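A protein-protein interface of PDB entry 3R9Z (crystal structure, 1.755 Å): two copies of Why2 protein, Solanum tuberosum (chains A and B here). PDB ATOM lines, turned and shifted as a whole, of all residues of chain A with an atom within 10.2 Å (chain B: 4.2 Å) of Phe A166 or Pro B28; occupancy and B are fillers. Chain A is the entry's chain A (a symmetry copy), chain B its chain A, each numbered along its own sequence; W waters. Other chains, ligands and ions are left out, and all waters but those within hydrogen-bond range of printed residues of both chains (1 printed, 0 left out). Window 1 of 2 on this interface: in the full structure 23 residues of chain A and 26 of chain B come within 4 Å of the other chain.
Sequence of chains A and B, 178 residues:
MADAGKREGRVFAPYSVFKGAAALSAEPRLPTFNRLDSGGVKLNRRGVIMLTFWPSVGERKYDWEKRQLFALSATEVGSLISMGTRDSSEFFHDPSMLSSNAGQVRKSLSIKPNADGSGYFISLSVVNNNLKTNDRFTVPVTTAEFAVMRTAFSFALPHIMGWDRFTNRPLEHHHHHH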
ATOM      1  N   PHE A  33      14.114  26.101  15.588  1.00  0.00           N
ATOM      2  CA  PHE A  33      14.872  25.047  14.943  1.00  0.00           C
ATOM      3  C   PHE A  33      16.315  25.494  14.773  1.00  0.00           C
ATOM      4  O   PHE A  33      16.598  26.692  14.700  1.00  0.00           O
ATOM      5  CB  PHE A  33      14.269  24.711  13.575  1.00  0.00           C
ATOM      6  CG  PHE A  33      13.010  23.879  13.649  1.00  0.00           C
ATOM      7  CD1 PHE A  33      11.773  24.476  13.823  1.00  0.00           C
ATOM      8  CD2 PHE A  33      13.074  22.497  13.527  1.00  0.00           C
ATOM      9  CE1 PHE A  33      10.620  23.709  13.891  1.00  0.00           C
ATOM     10  CE2 PHE A  33      11.925  21.723  13.592  1.00  0.00           C
ATOM     11  CZ  PHE A  33      10.701  22.330  13.771  1.00  0.00           C
ATOM     12  N   GLY A  40      19.295  20.344   6.358  1.00  0.00           N
ATOM     13  CA  GLY A  40      18.072  20.059   7.081  1.00  0.00           C
ATOM     14  C   GLY A  40      18.016  20.835   8.381  1.00  0.00           C
ATOM     15  O   GLY A  40      18.920  21.609   8.698  1.00  0.00           O
ATOM     16  N   VAL A  41      16.958  20.624   9.145  1.00  0.00           N
ATOM     17  CA  VAL A  41      16.786  21.346  10.393  1.00  0.00           C
ATOM     18  C   VAL A  41      16.491  20.382  11.531  1.00  0.00           C
ATOM     19  O   VAL A  41      16.086  19.248  11.300  1.00  0.00           O
ATOM     20  CB  VAL A  41      15.631  22.363  10.284  1.00  0.00           C
ATOM     21  CG1 VAL A  41      15.958  23.416   9.224  1.00  0.00           C
ATOM     22  CG2 VAL A  41      14.308  21.648   9.969  1.00  0.00           C
ATOM     23  N   LYS A  42      16.702  20.835  12.758  1.00  0.00           N
ATOM     24  CA  LYS A  42      16.372  20.028  13.924  1.00  0.00           C
ATOM     25  C   LYS A  42      15.801  20.898  15.036  1.00  0.00           C
ATOM     26  O   LYS A  42      16.300  21.993  15.299  1.00  0.00           O
ATOM     27  CB  LYS A  42      17.597  19.247  14.406  1.00  0.00           C
ATOM     28  CG  LYS A  42      18.679  20.083  15.046  1.00  0.00           C
ATOM     29  CD  LYS A  42      19.118  19.430  16.343  1.00  0.00           C
ATOM     30  CE  LYS A  42      19.236  17.921  16.171  1.00  0.00           C
ATOM     31  NZ  LYS A  42      19.111  17.194  17.464  1.00  0.00           N
ATOM     32  N   LEU A  43      14.738  20.422  15.682  1.00  0.00           N
ATOM     33  CA  LEU A  43      14.063  21.223  16.692  1.00  0.00           C
ATOM     34  C   LEU A  43      15.017  21.594  17.836  1.00  0.00           C
ATOM     35  O   LEU A  43      15.788  20.761  18.310  1.00  0.00           O
ATOM     36  CB  LEU A  43      12.819  20.494  17.215  1.00  0.00           C
ATOM     37  CG  LEU A  43      11.800  21.396  17.916  1.00  0.00           C
ATOM     38  CD1 LEU A  43      10.372  20.924  17.662  1.00  0.00           C
ATOM     39  CD2 LEU A  43      12.101  21.480  19.408  1.00  0.00           C
ATOM     40  N   PRO A 158       0.452  19.898  16.560  1.00  0.00           N
ATOM     41  CA  PRO A 158       1.442  19.466  15.566  1.00  0.00           C
ATOM     42  C   PRO A 158       2.381  20.611  15.225  1.00  0.00           C
ATOM     43  O   PRO A 158       3.552  20.371  15.014  1.00  0.00           O
ATOM     44  CB  PRO A 158       0.595  19.110  14.345  1.00  0.00           C
ATOM     45  CG  PRO A 158      -0.755  18.804  14.894  1.00  0.00           C
ATOM     46  CD  PRO A 158      -0.928  19.667  16.098  1.00  0.00           C
ATOM     47  N   HIS A 159       1.870  21.837  15.208  1.00  0.00           N
ATOM     48  CA  HIS A 159       2.707  23.009  14.963  1.00  0.00           C
ATOM     49  C   HIS A 159       3.715  23.259  16.093  1.00  0.00           C
ATOM     50  O   HIS A 159       4.906  23.458  15.832  1.00  0.00           O
ATOM     51  CB  HIS A 159       1.851  24.255  14.688  1.00  0.00           C
ATOM     52  CG  HIS A 159       0.960  24.113  13.490  1.00  0.00           C
ATOM     53  ND1 HIS A 159       1.428  24.223  12.198  1.00  0.00           N
ATOM     54  CD2 HIS A 159      -0.363  23.849  13.387  1.00  0.00           C
ATOM     55  CE1 HIS A 159       0.431  24.036  11.352  1.00  0.00           C
ATOM     56  NE2 HIS A 159      -0.669  23.813  12.048  1.00  0.00           N
ATOM     57  N   MET A 161       4.876  21.150  18.088  1.00  0.00           N
ATOM     58  CA  MET A 161       5.786  19.999  18.079  1.00  0.00           C
ATOM     59  C   MET A 161       6.770  20.018  16.909  1.00  0.00           C
ATOM     60  O   MET A 161       7.700  19.211  16.868  1.00  0.00           O
ATOM     61  CB  MET A 161       4.993  18.695  17.975  1.00  0.00           C
ATOM     62  CG  MET A 161       4.201  18.333  19.199  1.00  0.00           C
ATOM     63  SD  MET A 161       3.061  16.985  18.798  1.00  0.00           S
ATOM     64  CE  MET A 161       4.194  15.619  18.677  1.00  0.00           C
ATOM     65  N   GLY A 162       6.521  20.884  15.932  1.00  0.00           N
ATOM     66  CA  GLY A 162       7.339  20.940  14.729  1.00  0.00           C
ATOM     67  C   GLY A 162       6.960  19.930  13.652  1.00  0.00           C
ATOM     68  O   GLY A 162       7.654  19.790  12.648  1.00  0.00           O
ATOM     69  N   TRP A 163       5.845  19.228  13.843  1.00  0.00           N
ATOM     70  CA  TRP A 163       5.454  18.164  12.913  1.00  0.00           C
ATOM     71  C   TRP A 163       4.822  18.688  11.624  1.00  0.00           C
ATOM     72  O   TRP A 163       4.658  17.940  10.655  1.00  0.00           O
ATOM     73  CB  TRP A 163       4.515  17.166  13.600  1.00  0.00           C
ATOM     74  CG  TRP A 163       5.254  16.101  14.382  1.00  0.00           C
ATOM     75  CD1 TRP A 163       6.423  16.252  15.085  1.00  0.00           C
ATOM     76  CD2 TRP A 163       4.890  14.724  14.503  1.00  0.00           C
ATOM     77  NE1 TRP A 163       6.790  15.059  15.652  1.00  0.00           N
ATOM     78  CE2 TRP A 163       5.872  14.102  15.308  1.00  0.00           C
ATOM     79  CE3 TRP A 163       3.829  13.957  14.018  1.00  0.00           C
ATOM     80  CZ2 TRP A 163       5.816  12.748  15.639  1.00  0.00           C
ATOM     81  CZ3 TRP A 163       3.775  12.624  14.344  1.00  0.00           C
ATOM     82  CH2 TRP A 163       4.764  12.024  15.145  1.00  0.00           C
ATOM     83  N   ASP A 164       4.477  19.970  11.612  1.00  0.00           N
ATOM     84  CA  ASP A 164       3.964  20.602  10.393  1.00  0.00           C
ATOM     85  C   ASP A 164       5.037  20.693   9.312  1.00  0.00           C
ATOM     86  O   ASP A 164       4.737  20.959   8.149  1.00  0.00           O
ATOM     87  CB  ASP A 164       3.348  21.979  10.689  1.00  0.00           C
ATOM     88  CG  ASP A 164       4.330  22.950  11.351  1.00  0.00           C
ATOM     89  OD1 ASP A 164       5.354  22.512  11.918  1.00  0.00           O
ATOM     90  OD2 ASP A 164       4.061  24.167  11.319  1.00  0.00           O
ATOM     91  N   ARG A 165       6.287  20.462   9.705  1.00  0.00           N
ATOM     92  CA  ARG A 165       7.412  20.457   8.783  1.00  0.00           C
ATOM     93  C   ARG A 165       7.492  19.154   7.982  1.00  0.00           C
ATOM     94  O   ARG A 165       8.195  19.088   6.976  1.00  0.00           O
ATOM     95  CB  ARG A 165       8.721  20.684   9.542  1.00  0.00           C
ATOM     96  CG  ARG A 165       8.781  21.982  10.334  1.00  0.00           C
ATOM     97  CD  ARG A 165       9.128  23.161   9.452  1.00  0.00           C
ATOM     98  NE  ARG A 165      10.047  24.077  10.124  1.00  0.00           N
ATOM     99  CZ  ARG A 165      11.217  24.465   9.626  1.00  0.00           C
ATOM    100  NH1 ARG A 165      11.616  24.028   8.440  1.00  0.00           N
ATOM    101  NH2 ARG A 165      11.984  25.298  10.313  1.00  0.00           N
ATOM    102  N   PHE A 166       6.782  18.119   8.432  1.00  0.00           N
ATOM    103  CA  PHE A 166       6.695  16.865   7.677  1.00  0.00           C
ATOM    104  C   PHE A 166       5.493  16.891   6.726  1.00  0.00           C
ATOM    105  O   PHE A 166       4.406  16.416   7.066  1.00  0.00           O
ATOM    106  CB  PHE A 166       6.578  15.650   8.609  1.00  0.00           C
ATOM    107  CG  PHE A 166       7.757  15.452   9.527  1.00  0.00           C
ATOM    108  CD1 PHE A 166       7.648  15.725  10.886  1.00  0.00           C
ATOM    109  CD2 PHE A 166       8.958  14.964   9.043  1.00  0.00           C
ATOM    110  CE1 PHE A 166       8.723  15.531  11.738  1.00  0.00           C
ATOM    111  CE2 PHE A 166      10.040  14.765   9.891  1.00  0.00           C
ATOM    112  CZ  PHE A 166       9.922  15.049  11.238  1.00  0.00           C
ATOM    113  N   THR A 167       5.689  17.448   5.536  1.00  0.00           N
ATOM    114  CA  THR A 167       4.612  17.572   4.557  1.00  0.00           C
ATOM    115  C   THR A 167       5.135  17.357   3.139  1.00  0.00           C
ATOM    116  O   THR A 167       6.275  17.702   2.833  1.00  0.00           O
ATOM    117  CB  THR A 167       3.952  18.962   4.618  1.00  0.00           C
ATOM    118  OG1 THR A 167       4.939  19.971   4.368  1.00  0.00           O
ATOM    119  CG2 THR A 167       3.330  19.197   5.985  1.00  0.00           C
ATOM    120  N   ASN A 168       4.294  16.785   2.280  1.00  0.00           N
ATOM    121  CA  ASN A 168       4.640  16.589   0.879  1.00  0.00           C
ATOM    122  C   ASN A 168       4.436  17.863   0.063  1.00  0.00           C
ATOM    123  O   ASN A 168       5.070  18.054  -0.979  1.00  0.00           O
ATOM    124  CB  ASN A 168       3.825  15.439   0.276  1.00  0.00           C
ATOM    125  CG  ASN A 168       4.068  14.114   0.981  1.00  0.00           C
ATOM    126  OD1 ASN A 168       5.163  13.552   0.906  1.00  0.00           O
ATOM    127  ND2 ASN A 168       3.041  13.597   1.655  1.00  0.00           N
ATOM    128  N   VAL B  11      14.103  16.868   8.068  1.00  0.00           N
ATOM    129  CA  VAL B  11      13.579  17.503   9.269  1.00  0.00           C
ATOM    130  C   VAL B  11      13.717  16.528  10.418  1.00  0.00           C
ATOM    131  O   VAL B  11      13.383  15.350  10.270  1.00  0.00           O
ATOM    132  CB  VAL B  11      12.092  17.890   9.106  1.00  0.00           C
ATOM    133  CG1 VAL B  11      11.546  18.472  10.401  1.00  0.00           C
ATOM    134  CG2 VAL B  11      11.926  18.879   7.951  1.00  0.00           C
ATOM    135  N   ALA B  13      12.346  16.273  14.266  1.00  0.00           N
ATOM    136  CA  ALA B  13      11.520  16.822  15.331  1.00  0.00           C
ATOM    137  C   ALA B  13      10.739  15.702  16.001  1.00  0.00           C
ATOM    138  O   ALA B  13       9.511  15.675  15.967  1.00  0.00           O
ATOM    139  CB  ALA B  13      10.570  17.885  14.773  1.00  0.00           C
ATOM    140  N   GLU B  27       8.451   9.671  14.861  1.00  0.00           N
ATOM    141  CA  GLU B  27       8.639  10.657  13.820  1.00  0.00           C
ATOM    142  C   GLU B  27       8.029  10.134  12.526  1.00  0.00           C
ATOM    143  O   GLU B  27       8.200   8.956  12.192  1.00  0.00           O
ATOM    144  CB  GLU B  27      10.135  10.881  13.618  1.00  0.00           C
ATOM    145  CG  GLU B  27      10.507  12.215  13.065  1.00  0.00           C
ATOM    146  CD  GLU B  27      12.002  12.449  13.149  1.00  0.00           C
ATOM    147  OE1 GLU B  27      12.759  11.454  13.094  1.00  0.00           O
ATOM    148  OE2 GLU B  27      12.417  13.616  13.287  1.00  0.00           O
ATOM    149  N   PRO B  28       7.321  10.995  11.786  1.00  0.00           N
ATOM    150  CA  PRO B  28       6.816  10.543  10.481  1.00  0.00           C
ATOM    151  C   PRO B  28       7.933  10.347   9.460  1.00  0.00           C
ATOM    152  O   PRO B  28       8.943  11.053   9.519  1.00  0.00           O
ATOM    153  CB  PRO B  28       5.894  11.695  10.032  1.00  0.00           C
ATOM    154  CG  PRO B  28       5.631  12.505  11.270  1.00  0.00           C
ATOM    155  CD  PRO B  28       6.868  12.353  12.124  1.00  0.00           C
ATOM    156  N   ARG B  29       7.759   9.387   8.554  1.00  0.00           N
ATOM    157  CA  ARG B  29       8.548   9.308   7.329  1.00  0.00           C
ATOM    158  C   ARG B  29       7.603   9.448   6.135  1.00  0.00           C
ATOM    159  O   ARG B  29       6.682   8.647   5.956  1.00  0.00           O
ATOM    160  CB  ARG B  29       9.327   7.995   7.245  1.00  0.00           C
ATOM    161  CG  ARG B  29      10.333   7.961   6.092  1.00  0.00           C
ATOM    162  CD  ARG B  29      10.898   6.561   5.874  1.00  0.00           C
ATOM    163  NE  ARG B  29       9.947   5.683   5.193  1.00  0.00           N
ATOM    164  CZ  ARG B  29       9.905   4.362   5.341  1.00  0.00           C
ATOM    165  NH1 ARG B  29      10.748   3.756   6.169  1.00  0.00           N
ATOM    166  NH2 ARG B  29       9.007   3.645   4.671  1.00  0.00           N
ATOM    167  N   LEU B  30       7.823  10.474   5.326  1.00  0.00           N
ATOM    168  CA  LEU B  30       6.951  10.743   4.189  1.00  0.00           C
ATOM    169  C   LEU B  30       7.105   9.693   3.094  1.00  0.00           C
ATOM    170  O   LEU B  30       8.176   9.089   2.948  1.00  0.00           O
ATOM    171  CB  LEU B  30       7.255  12.130   3.613  1.00  0.00           C
ATOM    172  CG  LEU B  30       6.957  13.303   4.550  1.00  0.00           C
ATOM    173  CD1 LEU B  30       7.467  14.607   3.940  1.00  0.00           C
ATOM    174  CD2 LEU B  30       5.463  13.385   4.866  1.00  0.00           C
ATOM    175  N   VAL B  48       5.457   5.984   6.615  1.00  0.00           N
ATOM    176  CA  VAL B  48       5.232   5.314   7.898  1.00  0.00           C
ATOM    177  C   VAL B  48       5.368   6.317   9.053  1.00  0.00           C
ATOM    178  O   VAL B  48       5.793   7.456   8.853  1.00  0.00           O
ATOM    179  CB  VAL B  48       6.250   4.158   8.156  1.00  0.00           C
ATOM    180  CG1 VAL B  48       6.106   3.034   7.123  1.00  0.00           C
ATOM    181  CG2 VAL B  48       7.692   4.696   8.168  1.00  0.00           C
ATOM    182  N   ILE B  49       4.990   5.895  10.256  1.00  0.00           N
ATOM    183  CA  ILE B  49       5.455   6.587  11.459  1.00  0.00           C
ATOM    184  C   ILE B  49       6.509   5.681  12.084  1.00  0.00           C
ATOM    185  O   ILE B  49       6.197   4.556  12.469  1.00  0.00           O
ATOM    186  CB  ILE B  49       4.334   6.839  12.477  1.00  0.00           C
ATOM    187  CG1 ILE B  49       3.204   7.678  11.857  1.00  0.00           C
ATOM    188  CG2 ILE B  49       4.887   7.502  13.744  1.00  0.00           C
ATOM    189  CD1 ILE B  49       3.568   9.118  11.606  1.00  0.00           C
ATOM    190  N   ALA B 156      -0.504  13.489  11.021  1.00  0.00           N
ATOM    191  CA  ALA B 156       0.487  12.993  10.071  1.00  0.00           C
ATOM    192  C   ALA B 156      -0.084  11.984   9.069  1.00  0.00           C
ATOM    193  O   ALA B 156       0.469  11.795   7.987  1.00  0.00           O
ATOM    194  CB  ALA B 156       1.665  12.382  10.823  1.00  0.00           C
ATOM    195  N   HIS B 159      -0.671  12.939   5.508  1.00  0.00           N
ATOM    196  CA  HIS B 159       0.651  13.206   4.946  1.00  0.00           C
ATOM    197  C   HIS B 159       1.398  11.921   4.564  1.00  0.00           C
ATOM    198  O   HIS B 159       1.926  11.816   3.452  1.00  0.00           O
ATOM    199  CB  HIS B 159       1.488  14.084   5.890  1.00  0.00           C
ATOM    200  CG  HIS B 159       0.867  15.421   6.167  1.00  0.00           C
ATOM    201  ND1 HIS B 159       0.907  16.461   5.263  1.00  0.00           N
ATOM    202  CD2 HIS B 159       0.176  15.880   7.236  1.00  0.00           C
ATOM    203  CE1 HIS B 159       0.268  17.503   5.765  1.00  0.00           C
ATOM    204  NE2 HIS B 159      -0.180  17.179   6.964  1.00  0.00           N
HETATM  205  O   HOH W   1       8.105  17.273  18.722  1.00  0.00           O
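OE2 of Glu B27 lies within hydrogen-bond range of N of Ala B13 (2.8 Å).
The backbone carbonyl oxygen (O) of Pro A158 lies within hydrogen-bond range of the backbone NH (N) of Trp A163, 2.8 Å away.
O of Ala B13 sits at hydrogen-bond distance from NE1 of Trp A163 (2.8 Å).
The backbone carbonyl oxygen of His B159 is in hydrogen-bond range of the side-chain amide nitrogen of Asn A168, 2.8 Å away.
Among the printed residues, pairs that only touch across the chains: Val A41 with Val B11 (3.7 Å), Met A161 with Ala B13 (3.8 Å), Trp A163 with Glu B27 (3.96 Å), Trp A163 with Pro B28 (3.6 Å), Arg A165 with Val B11 (3.7 Å), Phe A166 with Val B11 (3.4 Å), Phe A166 with Glu B27 (3.4 Å), Phe A166 with Pro B28 (3.7 Å), Phe A166 with Leu B30 (3.9 Å), Phe A166 with His B159 (3.8 Å), Thr A167 with Leu B30 (3.5 Å), Thr A167 with His B159 (3.5 Å) and Asn A168 with Leu B30 (3.7 Å).
Position printed for both chains: 159.
Of the 15 pairs that touch across the chains among the printed residues, none has its exchanged pair printed and touching as well.
Of the 10 printed residues of chain B, 6 touch a printed residue of chain A.
Hydrophobic or aromatic side chains of chain B that line the printed part of chain A: Val B11, Ala B13, Pro B28, Leu B30 and His B159.
Hydrophobic or aromatic side chains of chain A that line the printed part of chain B: Trp A163 and Phe A166.
Among the printed residues, 15 pairs touch across the chains.
Among the printed residues, no Asp or Glu carboxylate lies within 4 Å of a Lys or Arg side-chain nitrogen of the other chain.
Printed residues of chain B within 4 Å of Val A41: Val B11.
Of the printed residues of chain B, Met A161 touches Ala B13 (3.8 Å).
Of the printed residues of chain B, Arg A165 touches Val B11 (3.7 Å).
Of the printed residues of chain B, Phe A166 touches Val B11 (3.4 Å), Glu B27 (3.4 Å), Pro B28 (3.7 Å), Leu B30 (3.9 Å) and His B159 (3.8 Å).
Printed residues of chain B within 4 Å of Asn A168: Leu B30 (3.7 Å) and His B159 (2.8 Å).
Val B11 touches just these residues of chain A: Val A41, Arg A165 and Phe A166.
Of the printed residues of chain A, Ala B13 touches Met A161 and Trp A163.
Pro B28 touches just these residues of chain A: Trp A163 (3.6 Å) and Phe A166 (3.7 Å).
Of the printed residues of chain A, His B159 touches Phe A166 (3.8 Å), Thr A167 (3.5 Å) and Asn A168 (2.8 Å).
The nearest printed residue of chain B that does not touch Asn A168 is Ala B156 (7.1 Å).
Water W1 bridges the backbone carbonyl oxygen (O) of Met A161 (2.7 Å) and the backbone carbonyl oxygen (O) of Ala B13 (3.5 Å).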
